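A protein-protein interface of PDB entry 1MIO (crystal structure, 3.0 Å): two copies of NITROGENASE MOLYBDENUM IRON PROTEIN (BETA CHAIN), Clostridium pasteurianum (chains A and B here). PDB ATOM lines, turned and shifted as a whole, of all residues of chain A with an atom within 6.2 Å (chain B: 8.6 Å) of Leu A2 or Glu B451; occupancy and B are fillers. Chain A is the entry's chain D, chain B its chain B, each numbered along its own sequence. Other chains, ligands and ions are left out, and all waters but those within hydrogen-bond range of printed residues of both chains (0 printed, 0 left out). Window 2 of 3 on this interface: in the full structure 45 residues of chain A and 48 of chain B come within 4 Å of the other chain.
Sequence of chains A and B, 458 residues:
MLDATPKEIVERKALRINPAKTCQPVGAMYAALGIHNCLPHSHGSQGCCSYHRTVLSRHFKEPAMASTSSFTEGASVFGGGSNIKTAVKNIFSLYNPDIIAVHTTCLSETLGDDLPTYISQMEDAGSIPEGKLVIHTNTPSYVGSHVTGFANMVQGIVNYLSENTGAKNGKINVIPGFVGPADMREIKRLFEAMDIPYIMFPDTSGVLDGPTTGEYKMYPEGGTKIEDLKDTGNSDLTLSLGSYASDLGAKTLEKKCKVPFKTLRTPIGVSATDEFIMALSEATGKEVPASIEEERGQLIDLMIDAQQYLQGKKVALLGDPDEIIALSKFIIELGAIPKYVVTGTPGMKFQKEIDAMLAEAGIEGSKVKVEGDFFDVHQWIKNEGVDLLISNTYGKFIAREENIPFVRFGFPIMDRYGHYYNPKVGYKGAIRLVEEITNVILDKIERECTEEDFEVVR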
ATOM      1  N   LEU A   2      -0.282 -17.529   4.352  1.00  0.00           N
ATOM      2  CA  LEU A   2      -0.445 -16.162   3.923  1.00  0.00           C
ATOM      3  C   LEU A   2      -0.962 -16.464   2.513  1.00  0.00           C
ATOM      4  O   LEU A   2      -0.355 -16.183   1.502  1.00  0.00           O
ATOM      5  CB  LEU A   2       0.966 -15.411   3.978  1.00  0.00           C
ATOM      6  CG  LEU A   2       1.889 -15.257   5.220  1.00  0.00           C
ATOM      7  CD1 LEU A   2       3.019 -14.362   4.874  1.00  0.00           C
ATOM      8  CD2 LEU A   2       1.271 -14.519   6.355  1.00  0.00           C
ATOM      9  N   ASP A   3      -2.175 -16.972   2.392  1.00  0.00           N
ATOM     10  CA  ASP A   3      -2.570 -17.721   1.195  1.00  0.00           C
ATOM     11  C   ASP A   3      -3.603 -17.364   0.092  1.00  0.00           C
ATOM     12  O   ASP A   3      -3.235 -16.501  -0.703  1.00  0.00           O
ATOM     13  CB  ASP A   3      -2.826 -19.130   1.819  1.00  0.00           C
ATOM     14  CG  ASP A   3      -3.982 -19.229   2.812  1.00  0.00           C
ATOM     15  OD1 ASP A   3      -5.103 -19.348   2.348  1.00  0.00           O
ATOM     16  OD2 ASP A   3      -3.774 -19.210   4.022  1.00  0.00           O
ATOM     17  N   ALA A   4      -4.726 -18.147  -0.085  1.00  0.00           N
ATOM     18  CA  ALA A   4      -5.887 -18.026  -0.992  1.00  0.00           C
ATOM     19  C   ALA A   4      -5.862 -17.421  -2.415  1.00  0.00           C
ATOM     20  O   ALA A   4      -6.864 -16.929  -2.950  1.00  0.00           O
ATOM     21  CB  ALA A   4      -7.004 -17.309  -0.251  1.00  0.00           C
ATOM     22  N   THR A   5      -4.673 -17.453  -3.025  1.00  0.00           N
ATOM     23  CA  THR A   5      -4.396 -17.051  -4.403  1.00  0.00           C
ATOM     24  C   THR A   5      -4.660 -18.316  -5.247  1.00  0.00           C
ATOM     25  O   THR A   5      -4.052 -19.359  -4.951  1.00  0.00           O
ATOM     26  CB  THR A   5      -2.911 -16.623  -4.506  1.00  0.00           C
ATOM     27  OG1 THR A   5      -2.631 -15.572  -3.555  1.00  0.00           O
ATOM     28  CG2 THR A   5      -2.595 -16.236  -5.929  1.00  0.00           C
ATOM     29  N   HIS A 378       2.874 -13.616  -7.426  1.00  0.00           N
ATOM     30  CA  HIS A 378       2.653 -14.760  -6.572  1.00  0.00           C
ATOM     31  C   HIS A 378       2.067 -15.974  -7.317  1.00  0.00           C
ATOM     32  O   HIS A 378       2.413 -17.126  -7.020  1.00  0.00           O
ATOM     33  CB  HIS A 378       1.707 -14.365  -5.463  1.00  0.00           C
ATOM     34  CG  HIS A 378       1.516 -15.359  -4.338  1.00  0.00           C
ATOM     35  ND1 HIS A 378       0.504 -15.316  -3.501  1.00  0.00           N
ATOM     36  CD2 HIS A 378       2.374 -16.368  -3.957  1.00  0.00           C
ATOM     37  CE1 HIS A 378       0.726 -16.253  -2.611  1.00  0.00           C
ATOM     38  NE2 HIS A 378       1.846 -16.877  -2.893  1.00  0.00           N
ATOM     39  N   LYS A 396       7.094  -9.494   1.347  1.00  0.00           N
ATOM     40  CA  LYS A 396       7.177 -10.419   2.475  1.00  0.00           C
ATOM     41  C   LYS A 396       6.057 -11.480   2.607  1.00  0.00           C
ATOM     42  O   LYS A 396       6.254 -12.605   3.091  1.00  0.00           O
ATOM     43  CB  LYS A 396       7.247  -9.600   3.784  1.00  0.00           C
ATOM     44  CG  LYS A 396       6.044  -8.685   3.988  1.00  0.00           C
ATOM     45  CD  LYS A 396       5.617  -8.380   5.394  1.00  0.00           C
ATOM     46  CE  LYS A 396       6.715  -7.733   6.144  1.00  0.00           C
ATOM     47  NZ  LYS A 396       6.160  -6.663   6.926  1.00  0.00           N
ATOM     48  N   PHE A 397       4.843 -11.145   2.178  1.00  0.00           N
ATOM     49  CA  PHE A 397       3.763 -12.088   2.238  1.00  0.00           C
ATOM     50  C   PHE A 397       4.019 -13.310   1.321  1.00  0.00           C
ATOM     51  O   PHE A 397       3.760 -14.463   1.682  1.00  0.00           O
ATOM     52  CB  PHE A 397       2.478 -11.310   1.883  1.00  0.00           C
ATOM     53  CG  PHE A 397       1.872 -10.509   3.043  1.00  0.00           C
ATOM     54  CD1 PHE A 397       1.231 -11.156   4.094  1.00  0.00           C
ATOM     55  CD2 PHE A 397       1.932  -9.118   3.079  1.00  0.00           C
ATOM     56  CE1 PHE A 397       0.665 -10.441   5.145  1.00  0.00           C
ATOM     57  CE2 PHE A 397       1.362  -8.409   4.136  1.00  0.00           C
ATOM     58  CZ  PHE A 397       0.731  -9.071   5.170  1.00  0.00           C
ATOM     59  N   ILE A 398       4.579 -13.117   0.120  1.00  0.00           N
ATOM     60  CA  ILE A 398       4.887 -14.204  -0.816  1.00  0.00           C
ATOM     61  C   ILE A 398       6.105 -14.959  -0.287  1.00  0.00           C
ATOM     62  O   ILE A 398       6.011 -16.160  -0.122  1.00  0.00           O
ATOM     63  CB  ILE A 398       5.202 -13.626  -2.202  1.00  0.00           C
ATOM     64  CG1 ILE A 398       4.059 -12.808  -2.736  1.00  0.00           C
ATOM     65  CG2 ILE A 398       5.518 -14.784  -3.129  1.00  0.00           C
ATOM     66  CD1 ILE A 398       4.580 -11.837  -3.779  1.00  0.00           C
ATOM     67  N   ALA A 399       7.191 -14.243   0.004  1.00  0.00           N
ATOM     68  CA  ALA A 399       8.402 -14.730   0.618  1.00  0.00           C
ATOM     69  C   ALA A 399       8.254 -15.585   1.872  1.00  0.00           C
ATOM     70  O   ALA A 399       9.216 -16.259   2.247  1.00  0.00           O
ATOM     71  CB  ALA A 399       9.316 -13.550   0.981  1.00  0.00           C
ATOM     72  N   ARG A 400       7.136 -15.582   2.606  1.00  0.00           N
ATOM     73  CA  ARG A 400       6.945 -16.444   3.790  1.00  0.00           C
ATOM     74  C   ARG A 400       6.056 -17.618   3.412  1.00  0.00           C
ATOM     75  O   ARG A 400       6.017 -18.646   4.086  1.00  0.00           O
ATOM     76  CB  ARG A 400       6.253 -15.704   4.970  1.00  0.00           C
ATOM     77  CG  ARG A 400       6.472 -16.251   6.397  1.00  0.00           C
ATOM     78  CD  ARG A 400       5.267 -16.767   7.187  1.00  0.00           C
ATOM     79  NE  ARG A 400       5.308 -16.144   8.499  1.00  0.00           N
ATOM     80  CZ  ARG A 400       4.834 -16.658   9.642  1.00  0.00           C
ATOM     81  NH1 ARG A 400       4.250 -17.850   9.771  1.00  0.00           N
ATOM     82  NH2 ARG A 400       4.893 -15.864  10.696  1.00  0.00           N
ATOM     83  N   GLU A 401       5.284 -17.461   2.352  1.00  0.00           N
ATOM     84  CA  GLU A 401       4.426 -18.507   1.936  1.00  0.00           C
ATOM     85  C   GLU A 401       5.233 -19.577   1.161  1.00  0.00           C
ATOM     86  O   GLU A 401       5.265 -20.792   1.422  1.00  0.00           O
ATOM     87  CB  GLU A 401       3.353 -17.734   1.194  1.00  0.00           C
ATOM     88  CG  GLU A 401       2.109 -18.541   0.902  1.00  0.00           C
ATOM     89  CD  GLU A 401       1.555 -19.448   2.011  1.00  0.00           C
ATOM     90  OE1 GLU A 401       1.826 -19.294   3.215  1.00  0.00           O
ATOM     91  OE2 GLU A 401       0.810 -20.345   1.631  1.00  0.00           O
ATOM     92  N   GLU B 446       9.355 -11.983  12.687  1.00  0.00           N
ATOM     93  CA  GLU B 446       8.605 -12.114  11.453  1.00  0.00           C
ATOM     94  C   GLU B 446       8.483 -13.555  10.940  1.00  0.00           C
ATOM     95  O   GLU B 446       7.536 -13.952  10.250  1.00  0.00           O
ATOM     96  CB  GLU B 446       9.277 -11.286  10.421  1.00  0.00           C
ATOM     97  CG  GLU B 446       9.100  -9.849  10.800  1.00  0.00           C
ATOM     98  CD  GLU B 446       8.119  -9.113   9.926  1.00  0.00           C
ATOM     99  OE1 GLU B 446       6.903  -9.319  10.024  1.00  0.00           O
ATOM    100  OE2 GLU B 446       8.607  -8.322   9.139  1.00  0.00           O
ATOM    101  N   ARG B 447       9.490 -14.361  11.277  1.00  0.00           N
ATOM    102  CA  ARG B 447       9.575 -15.738  10.867  1.00  0.00           C
ATOM    103  C   ARG B 447       8.772 -16.603  11.814  1.00  0.00           C
ATOM    104  O   ARG B 447       7.974 -17.427  11.394  1.00  0.00           O
ATOM    105  CB  ARG B 447      11.068 -16.069  10.848  1.00  0.00           C
ATOM    106  CG  ARG B 447      11.497 -17.519  10.581  1.00  0.00           C
ATOM    107  CD  ARG B 447      12.934 -17.795  10.116  1.00  0.00           C
ATOM    108  NE  ARG B 447      13.879 -17.145  11.002  1.00  0.00           N
ATOM    109  CZ  ARG B 447      14.661 -16.132  10.567  1.00  0.00           C
ATOM    110  NH1 ARG B 447      14.609 -15.683   9.285  1.00  0.00           N
ATOM    111  NH2 ARG B 447      15.476 -15.501  11.450  1.00  0.00           N
ATOM    112  N   GLU B 448       8.933 -16.418  13.118  1.00  0.00           N
ATOM    113  CA  GLU B 448       8.334 -17.321  14.095  1.00  0.00           C
ATOM    114  C   GLU B 448       6.967 -16.841  14.637  1.00  0.00           C
ATOM    115  O   GLU B 448       6.407 -17.487  15.536  1.00  0.00           O
ATOM    116  CB  GLU B 448       9.339 -17.565  15.319  1.00  0.00           C
ATOM    117  CG  GLU B 448      10.878 -17.840  15.284  1.00  0.00           C
ATOM    118  CD  GLU B 448      11.499 -18.834  14.258  1.00  0.00           C
ATOM    119  OE1 GLU B 448      10.911 -19.901  14.010  1.00  0.00           O
ATOM    120  OE2 GLU B 448      12.583 -18.553  13.703  1.00  0.00           O
ATOM    121  N   CYS B 449       6.372 -15.708  14.239  1.00  0.00           N
ATOM    122  CA  CYS B 449       5.039 -15.354  14.726  1.00  0.00           C
ATOM    123  C   CYS B 449       3.909 -16.195  14.073  1.00  0.00           C
ATOM    124  O   CYS B 449       4.104 -17.082  13.219  1.00  0.00           O
ATOM    125  CB  CYS B 449       4.823 -13.835  14.513  1.00  0.00           C
ATOM    126  SG  CYS B 449       5.065 -13.168  12.863  1.00  0.00           S
ATOM    127  N   THR B 450       2.664 -16.024  14.516  1.00  0.00           N
ATOM    128  CA  THR B 450       1.604 -16.799  13.923  1.00  0.00           C
ATOM    129  C   THR B 450       1.066 -15.957  12.743  1.00  0.00           C
ATOM    130  O   THR B 450       1.354 -14.764  12.634  1.00  0.00           O
ATOM    131  CB  THR B 450       0.591 -17.136  15.098  1.00  0.00           C
ATOM    132  OG1 THR B 450      -0.016 -15.926  15.489  1.00  0.00           O
ATOM    133  CG2 THR B 450       1.245 -17.731  16.349  1.00  0.00           C
ATOM    134  N   GLU B 451       0.277 -16.481  11.813  1.00  0.00           N
ATOM    135  CA  GLU B 451      -0.044 -15.744  10.604  1.00  0.00           C
ATOM    136  C   GLU B 451      -0.947 -14.501  10.769  1.00  0.00           C
ATOM    137  O   GLU B 451      -0.995 -13.610   9.903  1.00  0.00           O
ATOM    138  CB  GLU B 451      -0.642 -16.767   9.608  1.00  0.00           C
ATOM    139  CG  GLU B 451       0.442 -17.466   8.788  1.00  0.00           C
ATOM    140  CD  GLU B 451       0.051 -18.453   7.672  1.00  0.00           C
ATOM    141  OE1 GLU B 451      -1.038 -18.346   7.107  1.00  0.00           O
ATOM    142  OE2 GLU B 451       0.865 -19.324   7.349  1.00  0.00           O
ATOM    143  N   GLU B 452      -1.662 -14.455  11.906  1.00  0.00           N
ATOM    144  CA  GLU B 452      -2.495 -13.333  12.318  1.00  0.00           C
ATOM    145  C   GLU B 452      -1.663 -12.422  13.169  1.00  0.00           C
ATOM    146  O   GLU B 452      -2.172 -11.432  13.618  1.00  0.00           O
ATOM    147  CB  GLU B 452      -3.686 -13.711  13.181  1.00  0.00           C
ATOM    148  CG  GLU B 452      -3.896 -15.181  13.546  1.00  0.00           C
ATOM    149  CD  GLU B 452      -3.371 -15.648  14.908  1.00  0.00           C
ATOM    150  OE1 GLU B 452      -3.462 -14.861  15.862  1.00  0.00           O
ATOM    151  OE2 GLU B 452      -2.919 -16.803  15.019  1.00  0.00           O
ATOM    152  N   ASP B 453      -0.405 -12.715  13.454  1.00  0.00           N
ATOM    153  CA  ASP B 453       0.503 -11.878  14.216  1.00  0.00           C
ATOM    154  C   ASP B 453       1.541 -11.330  13.251  1.00  0.00           C
ATOM    155  O   ASP B 453       2.578 -10.773  13.618  1.00  0.00           O
ATOM    156  CB  ASP B 453       1.291 -12.649  15.273  1.00  0.00           C
ATOM    157  CG  ASP B 453       0.685 -13.172  16.573  1.00  0.00           C
ATOM    158  OD1 ASP B 453      -0.532 -13.085  16.778  1.00  0.00           O
ATOM    159  OD2 ASP B 453       1.473 -13.701  17.372  1.00  0.00           O
ATOM    160  N   PHE B 454       1.332 -11.520  11.975  1.00  0.00           N
ATOM    161  CA  PHE B 454       2.255 -11.032  10.986  1.00  0.00           C
ATOM    162  C   PHE B 454       1.830  -9.586  10.785  1.00  0.00           C
ATOM    163  O   PHE B 454       0.643  -9.319  10.685  1.00  0.00           O
ATOM    164  CB  PHE B 454       2.078 -11.945   9.760  1.00  0.00           C
ATOM    165  CG  PHE B 454       3.228 -11.907   8.788  1.00  0.00           C
ATOM    166  CD1 PHE B 454       4.477 -12.303   9.199  1.00  0.00           C
ATOM    167  CD2 PHE B 454       2.994 -11.469   7.515  1.00  0.00           C
ATOM    168  CE1 PHE B 454       5.512 -12.248   8.306  1.00  0.00           C
ATOM    169  CE2 PHE B 454       4.043 -11.422   6.636  1.00  0.00           C
ATOM    170  CZ  PHE B 454       5.303 -11.811   7.023  1.00  0.00           C
ATOM    171  N   GLU B 455       2.778  -8.668  10.773  1.00  0.00           N
ATOM    172  CA  GLU B 455       2.556  -7.236  10.683  1.00  0.00           C
ATOM    173  C   GLU B 455       3.024  -6.674   9.371  1.00  0.00           C
ATOM    174  O   GLU B 455       3.757  -7.343   8.671  1.00  0.00           O
ATOM    175  CB  GLU B 455       3.325  -6.467  11.754  1.00  0.00           C
ATOM    176  CG  GLU B 455       3.040  -6.769  13.234  1.00  0.00           C
ATOM    177  CD  GLU B 455       1.638  -6.476  13.754  1.00  0.00           C
ATOM    178  OE1 GLU B 455       0.877  -5.795  13.047  1.00  0.00           O
ATOM    179  OE2 GLU B 455       1.321  -6.929  14.868  1.00  0.00           O
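CD1 of Leu A2 touches CE2 of Phe B454, 3.6 Å away. Phe B454 touches Lys A396 (CE2 to CD, 3.6 Å). Phe A397 touches Phe B454. Arg B447 touches Arg A400 (O to NH2, 3.5 Å). Arg A400 touches Glu B451 (NH1 to CG, 3.95 Å). Phe B454 touches Arg A400 (CD1 to NH2, 3.9 Å).
Of chain B, only Glu B451 (3.0 Å) and Phe B454 (3.6 Å) come within 4 Å of Leu A2. Of chain A, only Leu A2 and Arg A400 come within 4 Å of Glu B451. Of the printed residues of chain B, Lys A396 touches Glu B446, Phe B454 and Glu B455. Of the printed residues of chain A, Glu B455 touches Lys A396 (3.0 Å). Asp B453 touches none of the printed residues of chain A. Glu A401 touches none of the printed residues of chain B. The nearest printed residue of chain B that does not touch Leu A2 is Glu B452 (6.3 Å). The nearest residue of chain A that does not touch Glu B451 is Asp A3 (4.2 Å). The nearest printed residue of chain A that does not touch Glu B446 is Leu A2 (7.0 Å).
Printed residues of chain B that touch a printed residue of chain A: Glu B446, Arg B447, Cys B449, Glu B451, Phe B454 and Glu B455. Of the 11 printed residues of chain A, 4 touch a printed residue of chain B. Printed residues of chain A that touch a printed residue of chain B: Leu A2, Lys A396, Phe A397 and Arg A400. Hydrophobic or aromatic side chains of chain A that line the printed part of chain B: Leu A2 and Phe A397.
N of Leu A2 lies within hydrogen-bond range of OE1 of Glu A401, at 3.0 Å. O of Glu B446 lies within hydrogen-bond range of SG of Cys B449. The side-chain sulfur of Cys B449 lies within hydrogen-bond range of the backbone carbonyl oxygen of Asp B453 (3.5 Å). The side-chain carboxylate (OE2) of Glu B448 lies within salt-bridge range of the guanidinium group (NE) of Arg B447 (3.3 Å).
NZ of Lys A396 is in salt-bridge range of OE2 of Glu B446, at 3.7 Å. OE1 of Glu B451 is in hydrogen-bond range of N of Leu A2, at 3.0 Å. The backbone carbonyl oxygen (O) of Cys B449 lies within hydrogen-bond range of the guanidinium group (NH2) of Arg A400, 2.9 Å away. The backbone carbonyl oxygen of Glu B446 sits at hydrogen-bond distance from the guanidinium group of Arg A400, at 3.3 Å. O of Glu B455 sits at hydrogen-bond distance from NZ of Lys A396, at 3.0 Å.
No position is printed for both chains. Of the 11 pairs that touch across the chains among the printed residues, none has its exchanged pair printed and touching as well.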
